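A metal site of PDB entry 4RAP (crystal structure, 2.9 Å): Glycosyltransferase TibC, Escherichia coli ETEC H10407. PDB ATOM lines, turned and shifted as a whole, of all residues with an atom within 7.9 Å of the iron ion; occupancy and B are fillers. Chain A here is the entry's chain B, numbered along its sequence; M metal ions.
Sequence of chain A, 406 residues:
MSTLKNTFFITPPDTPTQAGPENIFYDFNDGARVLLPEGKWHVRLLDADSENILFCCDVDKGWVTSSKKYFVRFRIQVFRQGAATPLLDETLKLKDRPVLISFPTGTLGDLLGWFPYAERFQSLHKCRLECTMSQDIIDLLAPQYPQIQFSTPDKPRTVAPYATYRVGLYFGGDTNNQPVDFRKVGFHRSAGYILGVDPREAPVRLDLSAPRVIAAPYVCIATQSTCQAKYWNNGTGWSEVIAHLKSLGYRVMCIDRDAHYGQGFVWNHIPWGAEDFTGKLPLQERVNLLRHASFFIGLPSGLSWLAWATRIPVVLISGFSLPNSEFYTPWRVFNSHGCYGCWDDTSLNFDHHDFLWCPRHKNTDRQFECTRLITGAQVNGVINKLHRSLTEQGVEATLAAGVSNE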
ATOM      1  N   ALA A 229      22.426 -11.954 -10.255  1.00  0.00           N
ATOM      2  CA  ALA A 229      23.355 -11.314  -9.324  1.00  0.00           C
ATOM      3  C   ALA A 229      23.810 -12.251  -8.203  1.00  0.00           C
ATOM      4  O   ALA A 229      24.915 -12.080  -7.676  1.00  0.00           O
ATOM      5  CB  ALA A 229      22.739 -10.053  -8.727  1.00  0.00           C
ATOM      6  N   GLY A 319      28.501 -11.411  -3.328  1.00  0.00           N
ATOM      7  CA  GLY A 319      29.030 -10.066  -3.497  1.00  0.00           C
ATOM      8  C   GLY A 319      27.911  -9.037  -3.563  1.00  0.00           C
ATOM      9  O   GLY A 319      28.108  -7.851  -3.257  1.00  0.00           O
ATOM     10  N   PHE A 320      26.707  -9.498  -3.896  1.00  0.00           N
ATOM     11  CA  PHE A 320      25.605  -8.573  -4.047  1.00  0.00           C
ATOM     12  C   PHE A 320      24.992  -8.196  -2.717  1.00  0.00           C
ATOM     13  O   PHE A 320      24.294  -7.191  -2.616  1.00  0.00           O
ATOM     14  CB  PHE A 320      24.615  -9.098  -5.047  1.00  0.00           C
ATOM     15  CG  PHE A 320      23.358  -9.597  -4.467  1.00  0.00           C
ATOM     16  CD1 PHE A 320      23.366 -10.608  -3.526  1.00  0.00           C
ATOM     17  CD2 PHE A 320      22.135  -9.113  -4.943  1.00  0.00           C
ATOM     18  CE1 PHE A 320      22.192 -11.113  -3.013  1.00  0.00           C
ATOM     19  CE2 PHE A 320      20.968  -9.605  -4.426  1.00  0.00           C
ATOM     20  CZ  PHE A 320      20.989 -10.597  -3.460  1.00  0.00           C
ATOM     21  N   CYS A 339      32.106  -2.706  -6.902  1.00  0.00           N
ATOM     22  CA  CYS A 339      30.675  -2.641  -6.460  1.00  0.00           C
ATOM     23  C   CYS A 339      30.446  -3.889  -5.559  1.00  0.00           C
ATOM     24  O   CYS A 339      31.076  -4.956  -5.751  1.00  0.00           O
ATOM     25  CB  CYS A 339      29.640  -2.500  -7.671  1.00  0.00           C
ATOM     26  SG  CYS A 339      27.879  -3.202  -7.634  1.00  0.00           S
ATOM     27  N   TYR A 340      29.661  -3.695  -4.489  1.00  0.00           N
ATOM     28  CA  TYR A 340      29.167  -4.798  -3.665  1.00  0.00           C
ATOM     29  C   TYR A 340      27.913  -4.331  -2.945  1.00  0.00           C
ATOM     30  O   TYR A 340      27.627  -3.119  -2.892  1.00  0.00           O
ATOM     31  CB  TYR A 340      30.210  -5.241  -2.667  1.00  0.00           C
ATOM     32  CG  TYR A 340      30.633  -4.144  -1.749  1.00  0.00           C
ATOM     33  CD1 TYR A 340      29.796  -3.710  -0.730  1.00  0.00           C
ATOM     34  CD2 TYR A 340      31.874  -3.552  -1.888  1.00  0.00           C
ATOM     35  CE1 TYR A 340      30.174  -2.697   0.125  1.00  0.00           C
ATOM     36  CE2 TYR A 340      32.272  -2.534  -1.030  1.00  0.00           C
ATOM     37  CZ  TYR A 340      31.418  -2.112  -0.025  1.00  0.00           C
ATOM     38  OH  TYR A 340      31.792  -1.120   0.825  1.00  0.00           O
ATOM     39  N   GLY A 341      27.126  -5.268  -2.432  1.00  0.00           N
ATOM     40  CA  GLY A 341      25.960  -4.913  -1.618  1.00  0.00           C
ATOM     41  C   GLY A 341      24.812  -4.183  -2.259  1.00  0.00           C
ATOM     42  O   GLY A 341      24.131  -3.438  -1.610  1.00  0.00           O
ATOM     43  N   CYS A 342      24.593  -4.403  -3.559  1.00  0.00           N
ATOM     44  CA  CYS A 342      23.394  -3.917  -4.311  1.00  0.00           C
ATOM     45  C   CYS A 342      22.169  -4.123  -3.321  1.00  0.00           C
ATOM     46  O   CYS A 342      21.416  -3.186  -2.972  1.00  0.00           O
ATOM     47  CB  CYS A 342      23.221  -4.725  -5.722  1.00  0.00           C
ATOM     48  SG  CYS A 342      24.694  -4.941  -6.946  1.00  0.00           S
ATOM     49  N   TRP A 343      22.069  -5.335  -2.773  1.00  0.00           N
ATOM     50  CA  TRP A 343      20.914  -5.813  -2.057  1.00  0.00           C
ATOM     51  C   TRP A 343      20.572  -5.135  -0.753  1.00  0.00           C
ATOM     52  O   TRP A 343      19.398  -5.073  -0.366  1.00  0.00           O
ATOM     53  CB  TRP A 343      21.074  -7.314  -1.857  1.00  0.00           C
ATOM     54  CG  TRP A 343      20.100  -7.933  -0.893  1.00  0.00           C
ATOM     55  CD1 TRP A 343      20.310  -8.241   0.439  1.00  0.00           C
ATOM     56  CD2 TRP A 343      18.728  -8.365  -1.179  1.00  0.00           C
ATOM     57  NE1 TRP A 343      19.182  -8.825   0.988  1.00  0.00           N
ATOM     58  CE2 TRP A 343      18.201  -8.921   0.066  1.00  0.00           C
ATOM     59  CE3 TRP A 343      17.920  -8.350  -2.300  1.00  0.00           C
ATOM     60  CZ2 TRP A 343      16.912  -9.421   0.161  1.00  0.00           C
ATOM     61  CZ3 TRP A 343      16.614  -8.867  -2.200  1.00  0.00           C
ATOM     62  CH2 TRP A 343      16.129  -9.402  -0.999  1.00  0.00           C
ATOM     63  N   LEU A 348      18.505   2.012  -3.355  1.00  0.00           N
ATOM     64  CA  LEU A 348      18.153   1.284  -4.575  1.00  0.00           C
ATOM     65  C   LEU A 348      16.931   0.425  -4.301  1.00  0.00           C
ATOM     66  O   LEU A 348      16.460   0.377  -3.182  1.00  0.00           O
ATOM     67  CB  LEU A 348      19.304   0.377  -5.003  1.00  0.00           C
ATOM     68  CG  LEU A 348      20.655   1.080  -5.170  1.00  0.00           C
ATOM     69  CD1 LEU A 348      21.783   0.084  -5.404  1.00  0.00           C
ATOM     70  CD2 LEU A 348      20.600   2.088  -6.310  1.00  0.00           C
ATOM     71  N   TRP A 357      18.977  -8.011 -13.215  1.00  0.00           N
ATOM     72  CA  TRP A 357      19.084  -6.760 -12.488  1.00  0.00           C
ATOM     73  C   TRP A 357      20.447  -6.535 -11.881  1.00  0.00           C
ATOM     74  O   TRP A 357      20.930  -7.369 -11.113  1.00  0.00           O
ATOM     75  CB  TRP A 357      18.008  -6.773 -11.413  1.00  0.00           C
ATOM     76  CG  TRP A 357      18.084  -5.681 -10.375  1.00  0.00           C
ATOM     77  CD1 TRP A 357      17.686  -4.346 -10.497  1.00  0.00           C
ATOM     78  CD2 TRP A 357      18.494  -5.822  -8.971  1.00  0.00           C
ATOM     79  NE1 TRP A 357      17.846  -3.664  -9.311  1.00  0.00           N
ATOM     80  CE2 TRP A 357      18.326  -4.497  -8.349  1.00  0.00           C
ATOM     81  CE3 TRP A 357      18.995  -6.851  -8.207  1.00  0.00           C
ATOM     82  CZ2 TRP A 357      18.640  -4.256  -7.028  1.00  0.00           C
ATOM     83  CZ3 TRP A 357      19.303  -6.596  -6.862  1.00  0.00           C
ATOM     84  CH2 TRP A 357      19.115  -5.328  -6.295  1.00  0.00           C
ATOM     85  N   CYS A 358      21.134  -5.479 -12.331  1.00  0.00           N
ATOM     86  CA  CYS A 358      22.263  -4.881 -11.592  1.00  0.00           C
ATOM     87  C   CYS A 358      21.953  -3.372 -11.524  1.00  0.00           C
ATOM     88  O   CYS A 358      21.988  -2.704 -12.540  1.00  0.00           O
ATOM     89  CB  CYS A 358      23.683  -5.125 -12.250  1.00  0.00           C
ATOM     90  SG  CYS A 358      25.157  -4.890 -11.149  1.00  0.00           S
ATOM     91  N   PRO A 359      21.628  -2.836 -10.322  1.00  0.00           N
ATOM     92  CA  PRO A 359      21.255  -1.434 -10.283  1.00  0.00           C
ATOM     93  C   PRO A 359      22.371  -0.471 -10.736  1.00  0.00           C
ATOM     94  O   PRO A 359      22.094   0.502 -11.447  1.00  0.00           O
ATOM     95  CB  PRO A 359      20.966  -1.194  -8.787  1.00  0.00           C
ATOM     96  CG  PRO A 359      20.737  -2.535  -8.196  1.00  0.00           C
ATOM     97  CD  PRO A 359      21.648  -3.434  -8.967  1.00  0.00           C
ATOM     98  N   ARG A 360      23.607  -0.704 -10.283  1.00  0.00           N
ATOM     99  CA  ARG A 360      24.712   0.182 -10.590  1.00  0.00           C
ATOM    100  C   ARG A 360      25.348  -0.006 -11.978  1.00  0.00           C
ATOM    101  O   ARG A 360      25.781   0.979 -12.576  1.00  0.00           O
ATOM    102  CB  ARG A 360      25.798   0.115  -9.513  1.00  0.00           C
ATOM    103  CG  ARG A 360      25.762   1.241  -8.475  1.00  0.00           C
ATOM    104  CD  ARG A 360      25.173   0.876  -7.109  1.00  0.00           C
ATOM    105  NE  ARG A 360      26.061   0.079  -6.243  1.00  0.00           N
ATOM    106  CZ  ARG A 360      25.859  -0.104  -4.932  1.00  0.00           C
ATOM    107  NH1 ARG A 360      24.832   0.472  -4.335  1.00  0.00           N
ATOM    108  NH2 ARG A 360      26.693  -0.865  -4.206  1.00  0.00           N
ATOM    109  N   HIS A 361      25.377  -1.243 -12.497  1.00  0.00           N
ATOM    110  CA  HIS A 361      26.145  -1.532 -13.745  1.00  0.00           C
ATOM    111  C   HIS A 361      25.500  -2.297 -14.869  1.00  0.00           C
ATOM    112  O   HIS A 361      26.201  -2.736 -15.786  1.00  0.00           O
ATOM    113  CB  HIS A 361      27.508  -2.140 -13.400  1.00  0.00           C
ATOM    114  CG  HIS A 361      28.312  -1.274 -12.499  1.00  0.00           C
ATOM    115  ND1 HIS A 361      28.592   0.009 -12.801  1.00  0.00           N
ATOM    116  CD2 HIS A 361      28.847  -1.505 -11.260  1.00  0.00           C
ATOM    117  CE1 HIS A 361      29.288   0.551 -11.807  1.00  0.00           C
ATOM    118  NE2 HIS A 361      29.439  -0.370 -10.856  1.00  0.00           N
ATOM    119  N   LYS A 362      24.186  -2.449 -14.850  1.00  0.00           N
ATOM    120  CA  LYS A 362      23.510  -3.204 -15.913  1.00  0.00           C
ATOM    121  C   LYS A 362      23.899  -2.664 -17.264  1.00  0.00           C
ATOM    122  O   LYS A 362      24.015  -1.452 -17.441  1.00  0.00           O
ATOM    123  CB  LYS A 362      21.982  -3.150 -15.749  1.00  0.00           C
ATOM    124  CG  LYS A 362      21.195  -3.867 -16.831  1.00  0.00           C
ATOM    125  CD  LYS A 362      19.759  -4.083 -16.372  1.00  0.00           C
ATOM    126  CE  LYS A 362      18.938  -4.990 -17.305  1.00  0.00           C
ATOM    127  NZ  LYS A 362      19.669  -6.245 -17.677  1.00  0.00           N
ATOM    128  N   ARG A 366      31.129  -3.547 -16.571  1.00  0.00           N
ATOM    129  CA  ARG A 366      31.253  -3.821 -15.114  1.00  0.00           C
ATOM    130  C   ARG A 366      30.099  -4.670 -14.493  1.00  0.00           C
ATOM    131  O   ARG A 366      30.104  -4.966 -13.286  1.00  0.00           O
ATOM    132  CB  ARG A 366      31.415  -2.523 -14.332  1.00  0.00           C
ATOM    133  CG  ARG A 366      32.604  -1.704 -14.761  1.00  0.00           C
ATOM    134  CD  ARG A 366      32.694  -0.421 -13.956  1.00  0.00           C
ATOM    135  NE  ARG A 366      32.954  -0.707 -12.565  1.00  0.00           N
ATOM    136  CZ  ARG A 366      32.838   0.187 -11.586  1.00  0.00           C
ATOM    137  NH1 ARG A 366      32.472   1.425 -11.861  1.00  0.00           N
ATOM    138  NH2 ARG A 366      33.109  -0.162 -10.331  1.00  0.00           N
ATOM    139  N   GLN A 367      29.128  -5.029 -15.311  1.00  0.00           N
ATOM    140  CA  GLN A 367      28.007  -5.778 -14.819  1.00  0.00           C
ATOM    141  C   GLN A 367      28.463  -7.015 -14.033  1.00  0.00           C
ATOM    142  O   GLN A 367      29.314  -7.785 -14.492  1.00  0.00           O
ATOM    143  CB  GLN A 367      27.104  -6.164 -15.967  1.00  0.00           C
ATOM    144  CG  GLN A 367      25.813  -6.795 -15.511  1.00  0.00           C
ATOM    145  CD  GLN A 367      24.731  -6.751 -16.573  1.00  0.00           C
ATOM    146  OE1 GLN A 367      24.990  -6.372 -17.733  1.00  0.00           O
ATOM    147  NE2 GLN A 367      23.509  -7.125 -16.187  1.00  0.00           N
ATOM    148  N   PHE A 368      27.901  -7.184 -12.856  1.00  0.00           N
ATOM    149  CA  PHE A 368      28.183  -8.285 -11.938  1.00  0.00           C
ATOM    150  C   PHE A 368      29.596  -8.373 -11.440  1.00  0.00           C
ATOM    151  O   PHE A 368      30.052  -9.430 -11.004  1.00  0.00           O
ATOM    152  CB  PHE A 368      27.680  -9.593 -12.458  1.00  0.00           C
ATOM    153  CG  PHE A 368      26.218  -9.577 -12.832  1.00  0.00           C
ATOM    154  CD1 PHE A 368      25.280  -9.072 -11.978  1.00  0.00           C
ATOM    155  CD2 PHE A 368      25.796 -10.161 -14.024  1.00  0.00           C
ATOM    156  CE1 PHE A 368      23.953  -9.085 -12.288  1.00  0.00           C
ATOM    157  CE2 PHE A 368      24.443 -10.188 -14.349  1.00  0.00           C
ATOM    158  CZ  PHE A 368      23.525  -9.650 -13.476  1.00  0.00           C
ATOM    159  N   GLU A 369      30.268  -7.220 -11.468  1.00  0.00           N
ATOM    160  CA  GLU A 369      31.575  -7.064 -10.860  1.00  0.00           C
ATOM    161  C   GLU A 369      31.542  -7.580  -9.407  1.00  0.00           C
ATOM    162  O   GLU A 369      32.557  -8.006  -8.880  1.00  0.00           O
ATOM    163  CB  GLU A 369      31.943  -5.584 -10.926  1.00  0.00           C
ATOM    164  CG  GLU A 369      33.164  -5.171 -10.141  1.00  0.00           C
ATOM    165  CD  GLU A 369      33.603  -3.751 -10.484  1.00  0.00           C
ATOM    166  OE1 GLU A 369      33.109  -2.775  -9.882  1.00  0.00           O
ATOM    167  OE2 GLU A 369      34.450  -3.615 -11.382  1.00  0.00           O
ATOM    168  N   CYS A 370      30.342  -7.530  -8.799  1.00  0.00           N
ATOM    169  CA  CYS A 370      30.058  -8.031  -7.443  1.00  0.00           C
ATOM    170  C   CYS A 370      30.834  -9.371  -7.255  1.00  0.00           C
ATOM    171  O   CYS A 370      31.590  -9.556  -6.300  1.00  0.00           O
ATOM    172  CB  CYS A 370      28.486  -8.259  -7.202  1.00  0.00           C
ATOM    173  SG  CYS A 370      27.228  -7.011  -7.834  1.00  0.00           S
ATOM    174  N   THR A 371      30.661 -10.287  -8.208  1.00  0.00           N
ATOM    175  CA  THR A 371      31.170 -11.658  -8.066  1.00  0.00           C
ATOM    176  C   THR A 371      32.322 -12.024  -8.997  1.00  0.00           C
ATOM    177  O   THR A 371      33.040 -13.005  -8.731  1.00  0.00           O
ATOM    178  CB  THR A 371      30.037 -12.713  -8.201  1.00  0.00           C
ATOM    179  OG1 THR A 371      29.029 -12.221  -9.083  1.00  0.00           O
ATOM    180  CG2 THR A 371      29.387 -12.935  -6.888  1.00  0.00           C
HETATM  181 FE    FE M   1      26.031  -5.204  -8.724  1.00  0.00          FE
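The side-chain sulfur (SG) of Cys 342 is bound to the iron ion.
The side-chain sulfur (SG) of Cys 370 is bound to the iron ion.
SG of Cys 358 binds the iron ion (2.6 Å).
Slightly farther from the iron ion lies the side-chain sulfur (SG) of Cys 339 (2.9 Å).
The backbone NH (N) of Cys 342 lies within hydrogen-bond range of the backbone carbonyl oxygen (O) of Phe 320 (3.0 Å).
SG of Cys 339 lies close to SG of Cys 342 (3.7 Å).
The backbone NH (N) of Cys 339 sits at hydrogen-bond distance from the side-chain carboxylate (OE1) of Glu 369 (3.1 Å).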
